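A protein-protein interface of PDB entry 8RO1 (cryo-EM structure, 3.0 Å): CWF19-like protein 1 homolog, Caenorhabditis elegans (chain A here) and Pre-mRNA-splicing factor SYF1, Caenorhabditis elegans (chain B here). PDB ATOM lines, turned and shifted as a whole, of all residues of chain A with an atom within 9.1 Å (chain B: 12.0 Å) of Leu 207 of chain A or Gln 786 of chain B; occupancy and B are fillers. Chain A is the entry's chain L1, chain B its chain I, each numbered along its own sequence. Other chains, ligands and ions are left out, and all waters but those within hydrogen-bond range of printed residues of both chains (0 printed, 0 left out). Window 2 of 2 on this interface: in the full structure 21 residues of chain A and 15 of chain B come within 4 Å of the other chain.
NH2 of Arg 260 of chain A lies within hydrogen-bond range of O of Ser 788 of chain B (3.4 Å).
The backbone carbonyl oxygen (O) of Val 205 of chain A is in hydrogen-bond range of the side-chain hydroxyl (OG) of Ser 788 of chain B (2.8 Å).
N of Val 205 of chain A sits at hydrogen-bond distance from OE2 of Glu 256 of chain A (3.0 Å).
OE2 of Glu 256 of chain A is in salt-bridge range of NH1 of Arg 260 of chain A (3.995 Å).
The guanidinium group of Arg 204 of chain A is in salt-bridge range of the side-chain carboxylate of Glu 264 of chain A (2.6 Å).
Arg 204 of chain A touches Ser 788 of chain B (CB to OG, 3.8 Å).
O of Gln 786 of chain B touches CD2 of Leu 207 of chain A, 3.2 Å away.
Asn 790 of chain B touches Glu 256 of chain A.
CA of Met 789 of chain B touches NH1 of Arg 260 of chain A, at 3.8 Å.
Arg 204 of chain A touches just one residue of chain B: Ser 788.
No residue of chain B comes within 4 Å of Leu 206 of chain A.
Of the printed residues of chain B, Leu 207 of chain A touches Gln 786.
No residue of chain B comes within 4 Å of Glu 208 of chain A.
No residue of chain B comes within 4 Å of Pro 209 of chain A.
Printed residues of chain B within 4 Å of Glu 256 of chain A: Asn 790 (3.3 Å).
Of the printed residues of chain B, Arg 260 of chain A touches Ser 788 (3.4 Å) and Met 789 (3.8 Å).
Of chain A, only Leu 207 comes within 4 Å of Gln 786 of chain B.
No residue of chain A comes within 4 Å of Val 787 of chain B.
Of the printed residues of chain A, Ser 788 of chain B touches Arg 204 (3.8 Å), Val 205 (2.8 Å) and Arg 260 (3.4 Å).
Of the printed residues of chain A, Met 789 of chain B touches Arg 260 (3.8 Å).
Printed residues of chain A within 4 Å of Asn 790 of chain B: Glu 256.
The nearest printed residue of chain A that does not touch Asn 790 of chain B is Arg 260 of chain A (4.3 Å).
Printed residues of chain B that touch a printed residue of chain A: Gln 786, Ser 788, Met 789 and Asn 790.
Among the printed residues, 6 pairs touch across the chains.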
ATOM      1  N   HIS A 203      -6.494   0.462  27.293  1.00  0.00           N
ATOM      2  CA  HIS A 203      -5.267   1.180  26.988  1.00  0.00           C
ATOM      3  C   HIS A 203      -5.067   2.185  28.104  1.00  0.00           C
ATOM      4  O   HIS A 203      -5.961   2.419  28.919  1.00  0.00           O
ATOM      5  CB  HIS A 203      -5.359   1.904  25.657  1.00  0.00           C
ATOM      6  CG  HIS A 203      -6.673   2.570  25.454  1.00  0.00           C
ATOM      7  ND1 HIS A 203      -7.075   3.651  26.204  1.00  0.00           N
ATOM      8  CD2 HIS A 203      -7.701   2.284  24.626  1.00  0.00           C
ATOM      9  CE1 HIS A 203      -8.284   4.021  25.829  1.00  0.00           C
ATOM     10  NE2 HIS A 203      -8.690   3.202  24.877  1.00  0.00           N
ATOM     11  N   ARG A 204      -3.891   2.790  28.132  1.00  0.00           N
ATOM     12  CA  ARG A 204      -3.770   4.047  28.845  1.00  0.00           C
ATOM     13  C   ARG A 204      -4.676   5.058  28.156  1.00  0.00           C
ATOM     14  O   ARG A 204      -4.954   4.940  26.960  1.00  0.00           O
ATOM     15  CB  ARG A 204      -2.313   4.502  28.891  1.00  0.00           C
ATOM     16  CG  ARG A 204      -1.362   3.432  29.440  1.00  0.00           C
ATOM     17  CD  ARG A 204       0.090   3.829  29.365  1.00  0.00           C
ATOM     18  NE  ARG A 204       0.931   2.652  29.572  1.00  0.00           N
ATOM     19  CZ  ARG A 204       1.832   2.471  30.533  1.00  0.00           C
ATOM     20  NH1 ARG A 204       2.396   1.275  30.668  1.00  0.00           N
ATOM     21  NH2 ARG A 204       2.221   3.455  31.334  1.00  0.00           N
ATOM     22  N   VAL A 205      -5.192   6.020  28.923  1.00  0.00           N
ATOM     23  CA  VAL A 205      -5.937   7.127  28.334  1.00  0.00           C
ATOM     24  C   VAL A 205      -4.976   8.215  27.861  1.00  0.00           C
ATOM     25  O   VAL A 205      -3.836   8.323  28.315  1.00  0.00           O
ATOM     26  CB  VAL A 205      -6.975   7.664  29.344  1.00  0.00           C
ATOM     27  CG1 VAL A 205      -6.338   8.524  30.438  1.00  0.00           C
ATOM     28  CG2 VAL A 205      -8.120   8.416  28.655  1.00  0.00           C
ATOM     29  N   LEU A 206      -5.453   9.026  26.916  1.00  0.00           N
ATOM     30  CA  LEU A 206      -4.702  10.093  26.250  1.00  0.00           C
ATOM     31  C   LEU A 206      -3.450   9.702  25.457  1.00  0.00           C
ATOM     32  O   LEU A 206      -2.943  10.537  24.705  1.00  0.00           O
ATOM     33  CB  LEU A 206      -4.289  11.171  27.257  1.00  0.00           C
ATOM     34  CG  LEU A 206      -5.365  11.845  28.114  1.00  0.00           C
ATOM     35  CD1 LEU A 206      -4.756  13.040  28.830  1.00  0.00           C
ATOM     36  CD2 LEU A 206      -6.593  12.256  27.324  1.00  0.00           C
ATOM     37  N   LEU A 207      -2.885   8.513  25.648  1.00  0.00           N
ATOM     38  CA  LEU A 207      -1.654   8.129  24.976  1.00  0.00           C
ATOM     39  C   LEU A 207      -1.898   7.477  23.626  1.00  0.00           C
ATOM     40  O   LEU A 207      -1.046   7.590  22.738  1.00  0.00           O
ATOM     41  CB  LEU A 207      -0.843   7.184  25.864  1.00  0.00           C
ATOM     42  CG  LEU A 207       0.008   7.882  26.931  1.00  0.00           C
ATOM     43  CD1 LEU A 207       0.425   6.896  27.998  1.00  0.00           C
ATOM     44  CD2 LEU A 207       1.244   8.545  26.329  1.00  0.00           C
ATOM     45  N   GLU A 208      -3.030   6.794  23.456  1.00  0.00           N
ATOM     46  CA  GLU A 208      -3.274   5.895  22.338  1.00  0.00           C
ATOM     47  C   GLU A 208      -4.756   5.919  22.000  1.00  0.00           C
ATOM     48  O   GLU A 208      -5.571   6.223  22.878  1.00  0.00           O
ATOM     49  CB  GLU A 208      -2.850   4.457  22.663  1.00  0.00           C
ATOM     50  CG  GLU A 208      -1.352   4.257  22.803  1.00  0.00           C
ATOM     51  CD  GLU A 208      -0.983   2.811  23.067  1.00  0.00           C
ATOM     52  OE1 GLU A 208      -1.559   1.919  22.409  1.00  0.00           O
ATOM     53  OE2 GLU A 208      -0.119   2.566  23.935  1.00  0.00           O
ATOM     54  N   PRO A 209      -5.139   5.646  20.743  1.00  0.00           N
ATOM     55  CA  PRO A 209      -6.548   5.780  20.347  1.00  0.00           C
ATOM     56  C   PRO A 209      -7.488   4.905  21.159  1.00  0.00           C
ATOM     57  O   PRO A 209      -7.090   3.925  21.788  1.00  0.00           O
ATOM     58  CB  PRO A 209      -6.544   5.338  18.882  1.00  0.00           C
ATOM     59  CG  PRO A 209      -5.212   5.649  18.410  1.00  0.00           C
ATOM     60  CD  PRO A 209      -4.305   5.353  19.561  1.00  0.00           C
ATOM     61  N   ALA A 210      -8.757   5.292  21.151  1.00  0.00           N
ATOM     62  CA  ALA A 210      -9.772   4.569  21.901  1.00  0.00           C
ATOM     63  C   ALA A 210      -9.946   3.147  21.369  1.00  0.00           C
ATOM     64  O   ALA A 210      -9.791   2.881  20.174  1.00  0.00           O
ATOM     65  CB  ALA A 210     -11.106   5.313  21.839  1.00  0.00           C
ATOM     66  N   GLN A 250     -16.618   5.472  23.992  1.00  0.00           N
ATOM     67  CA  GLN A 250     -16.367   5.079  25.371  1.00  0.00           C
ATOM     68  C   GLN A 250     -17.620   5.290  26.215  1.00  0.00           C
ATOM     69  O   GLN A 250     -17.995   6.444  26.451  1.00  0.00           O
ATOM     70  CB  GLN A 250     -15.212   5.888  25.959  1.00  0.00           C
ATOM     71  CG  GLN A 250     -13.848   5.548  25.374  1.00  0.00           C
ATOM     72  CD  GLN A 250     -12.702   6.215  26.118  1.00  0.00           C
ATOM     73  OE1 GLN A 250     -12.849   6.629  27.268  1.00  0.00           O
ATOM     74  NE2 GLN A 250     -11.554   6.328  25.459  1.00  0.00           N
ATOM     75  N   GLU A 256      -9.888   3.230  33.906  1.00  0.00           N
ATOM     76  CA  GLU A 256      -8.593   2.798  33.384  1.00  0.00           C
ATOM     77  C   GLU A 256      -8.387   1.290  33.562  1.00  0.00           C
ATOM     78  O   GLU A 256      -9.048   0.632  34.369  1.00  0.00           O
ATOM     79  CB  GLU A 256      -7.458   3.544  34.077  1.00  0.00           C
ATOM     80  CG  GLU A 256      -7.373   5.025  33.736  1.00  0.00           C
ATOM     81  CD  GLU A 256      -7.237   5.322  32.255  1.00  0.00           C
ATOM     82  OE1 GLU A 256      -8.289   5.429  31.586  1.00  0.00           O
ATOM     83  OE2 GLU A 256      -6.097   5.466  31.771  1.00  0.00           O
ATOM     84  N   ARG A 260      -3.232  -3.102  34.121  1.00  0.00           N
ATOM     85  CA  ARG A 260      -2.091  -2.390  33.559  1.00  0.00           C
ATOM     86  C   ARG A 260      -0.890  -2.480  34.486  1.00  0.00           C
ATOM     87  O   ARG A 260       0.220  -2.804  34.054  1.00  0.00           O
ATOM     88  CB  ARG A 260      -2.462  -0.926  33.310  1.00  0.00           C
ATOM     89  CG  ARG A 260      -1.452  -0.151  32.469  1.00  0.00           C
ATOM     90  CD  ARG A 260      -0.892   1.065  33.186  1.00  0.00           C
ATOM     91  NE  ARG A 260      -1.844   2.169  33.122  1.00  0.00           N
ATOM     92  CZ  ARG A 260      -1.552   3.450  33.312  1.00  0.00           C
ATOM     93  NH1 ARG A 260      -2.495   4.365  33.103  1.00  0.00           N
ATOM     94  NH2 ARG A 260      -0.365   3.838  33.751  1.00  0.00           N
ATOM     95  N   GLU A 264       2.761  -5.190  34.079  1.00  0.00           N
ATOM     96  CA  GLU A 264       4.157  -4.778  34.135  1.00  0.00           C
ATOM     97  C   GLU A 264       4.903  -5.547  35.218  1.00  0.00           C
ATOM     98  O   GLU A 264       6.070  -5.915  35.040  1.00  0.00           O
ATOM     99  CB  GLU A 264       4.239  -3.272  34.374  1.00  0.00           C
ATOM    100  CG  GLU A 264       3.794  -2.440  33.178  1.00  0.00           C
ATOM    101  CD  GLU A 264       3.803  -0.952  33.461  1.00  0.00           C
ATOM    102  OE1 GLU A 264       4.245  -0.554  34.560  1.00  0.00           O
ATOM    103  OE2 GLU A 264       3.368  -0.176  32.584  1.00  0.00           O
ATOM    104  N   THR B 785       5.261  13.492  24.591  1.00  0.00           N
ATOM    105  CA  THR B 785       3.908  13.584  25.114  1.00  0.00           C
ATOM    106  C   THR B 785       3.891  13.097  26.548  1.00  0.00           C
ATOM    107  O   THR B 785       4.908  12.654  27.066  1.00  0.00           O
ATOM    108  CB  THR B 785       2.918  12.756  24.252  1.00  0.00           C
ATOM    109  OG1 THR B 785       3.415  11.423  24.087  1.00  0.00           O
ATOM    110  CG2 THR B 785       2.722  13.398  22.886  1.00  0.00           C
ATOM    111  N   GLN B 786       2.732  13.184  27.184  1.00  0.00           N
ATOM    112  CA  GLN B 786       2.611  13.043  28.625  1.00  0.00           C
ATOM    113  C   GLN B 786       2.100  11.655  28.958  1.00  0.00           C
ATOM    114  O   GLN B 786       1.214  11.133  28.275  1.00  0.00           O
ATOM    115  CB  GLN B 786       1.654  14.092  29.199  1.00  0.00           C
ATOM    116  CG  GLN B 786       1.840  14.385  30.685  1.00  0.00           C
ATOM    117  CD  GLN B 786       3.152  15.076  30.997  1.00  0.00           C
ATOM    118  OE1 GLN B 786       3.705  15.797  30.166  1.00  0.00           O
ATOM    119  NE2 GLN B 786       3.669  14.840  32.196  1.00  0.00           N
ATOM    120  N   VAL B 787       2.654  11.067  30.010  1.00  0.00           N
ATOM    121  CA  VAL B 787       2.270   9.728  30.439  1.00  0.00           C
ATOM    122  C   VAL B 787       1.176   9.877  31.481  1.00  0.00           C
ATOM    123  O   VAL B 787       1.391  10.481  32.535  1.00  0.00           O
ATOM    124  CB  VAL B 787       3.467   8.947  31.001  1.00  0.00           C
ATOM    125  CG1 VAL B 787       3.103   7.460  31.160  1.00  0.00           C
ATOM    126  CG2 VAL B 787       4.711   9.117  30.127  1.00  0.00           C
ATOM    127  N   SER B 788       0.007   9.319  31.200  1.00  0.00           N
ATOM    128  CA  SER B 788      -1.034   9.214  32.208  1.00  0.00           C
ATOM    129  C   SER B 788      -0.749   8.081  33.187  1.00  0.00           C
ATOM    130  O   SER B 788      -0.070   7.103  32.871  1.00  0.00           O
ATOM    131  CB  SER B 788      -2.398   8.998  31.549  1.00  0.00           C
ATOM    132  OG  SER B 788      -2.380   7.867  30.695  1.00  0.00           O
ATOM    133  N   MET B 789      -1.270   8.245  34.395  1.00  0.00           N
ATOM    134  CA  MET B 789      -1.324   7.203  35.402  1.00  0.00           C
ATOM    135  C   MET B 789      -2.550   7.505  36.237  1.00  0.00           C
ATOM    136  O   MET B 789      -2.920   8.670  36.394  1.00  0.00           O
ATOM    137  CB  MET B 789      -0.055   7.182  36.261  1.00  0.00           C
ATOM    138  CG  MET B 789      -0.122   6.330  37.532  1.00  0.00           C
ATOM    139  SD  MET B 789       1.410   6.378  38.475  1.00  0.00           S
ATOM    140  CE  MET B 789       1.249   7.973  39.279  1.00  0.00           C
ATOM    141  N   ASN B 790      -3.176   6.469  36.774  1.00  0.00           N
ATOM    142  CA  ASN B 790      -4.393   6.638  37.550  1.00  0.00           C
ATOM    143  C   ASN B 790      -4.121   6.591  39.046  1.00  0.00           C
ATOM    144  O   ASN B 790      -3.133   6.020  39.502  1.00  0.00           O
ATOM    145  CB  ASN B 790      -5.415   5.563  37.204  1.00  0.00           C
ATOM    146  CG  ASN B 790      -6.797   5.919  37.673  1.00  0.00           C
ATOM    147  OD1 ASN B 790      -7.135   5.727  38.836  1.00  0.00           O
ATOM    148  ND2 ASN B 790      -7.617   6.433  36.764  1.00  0.00           N
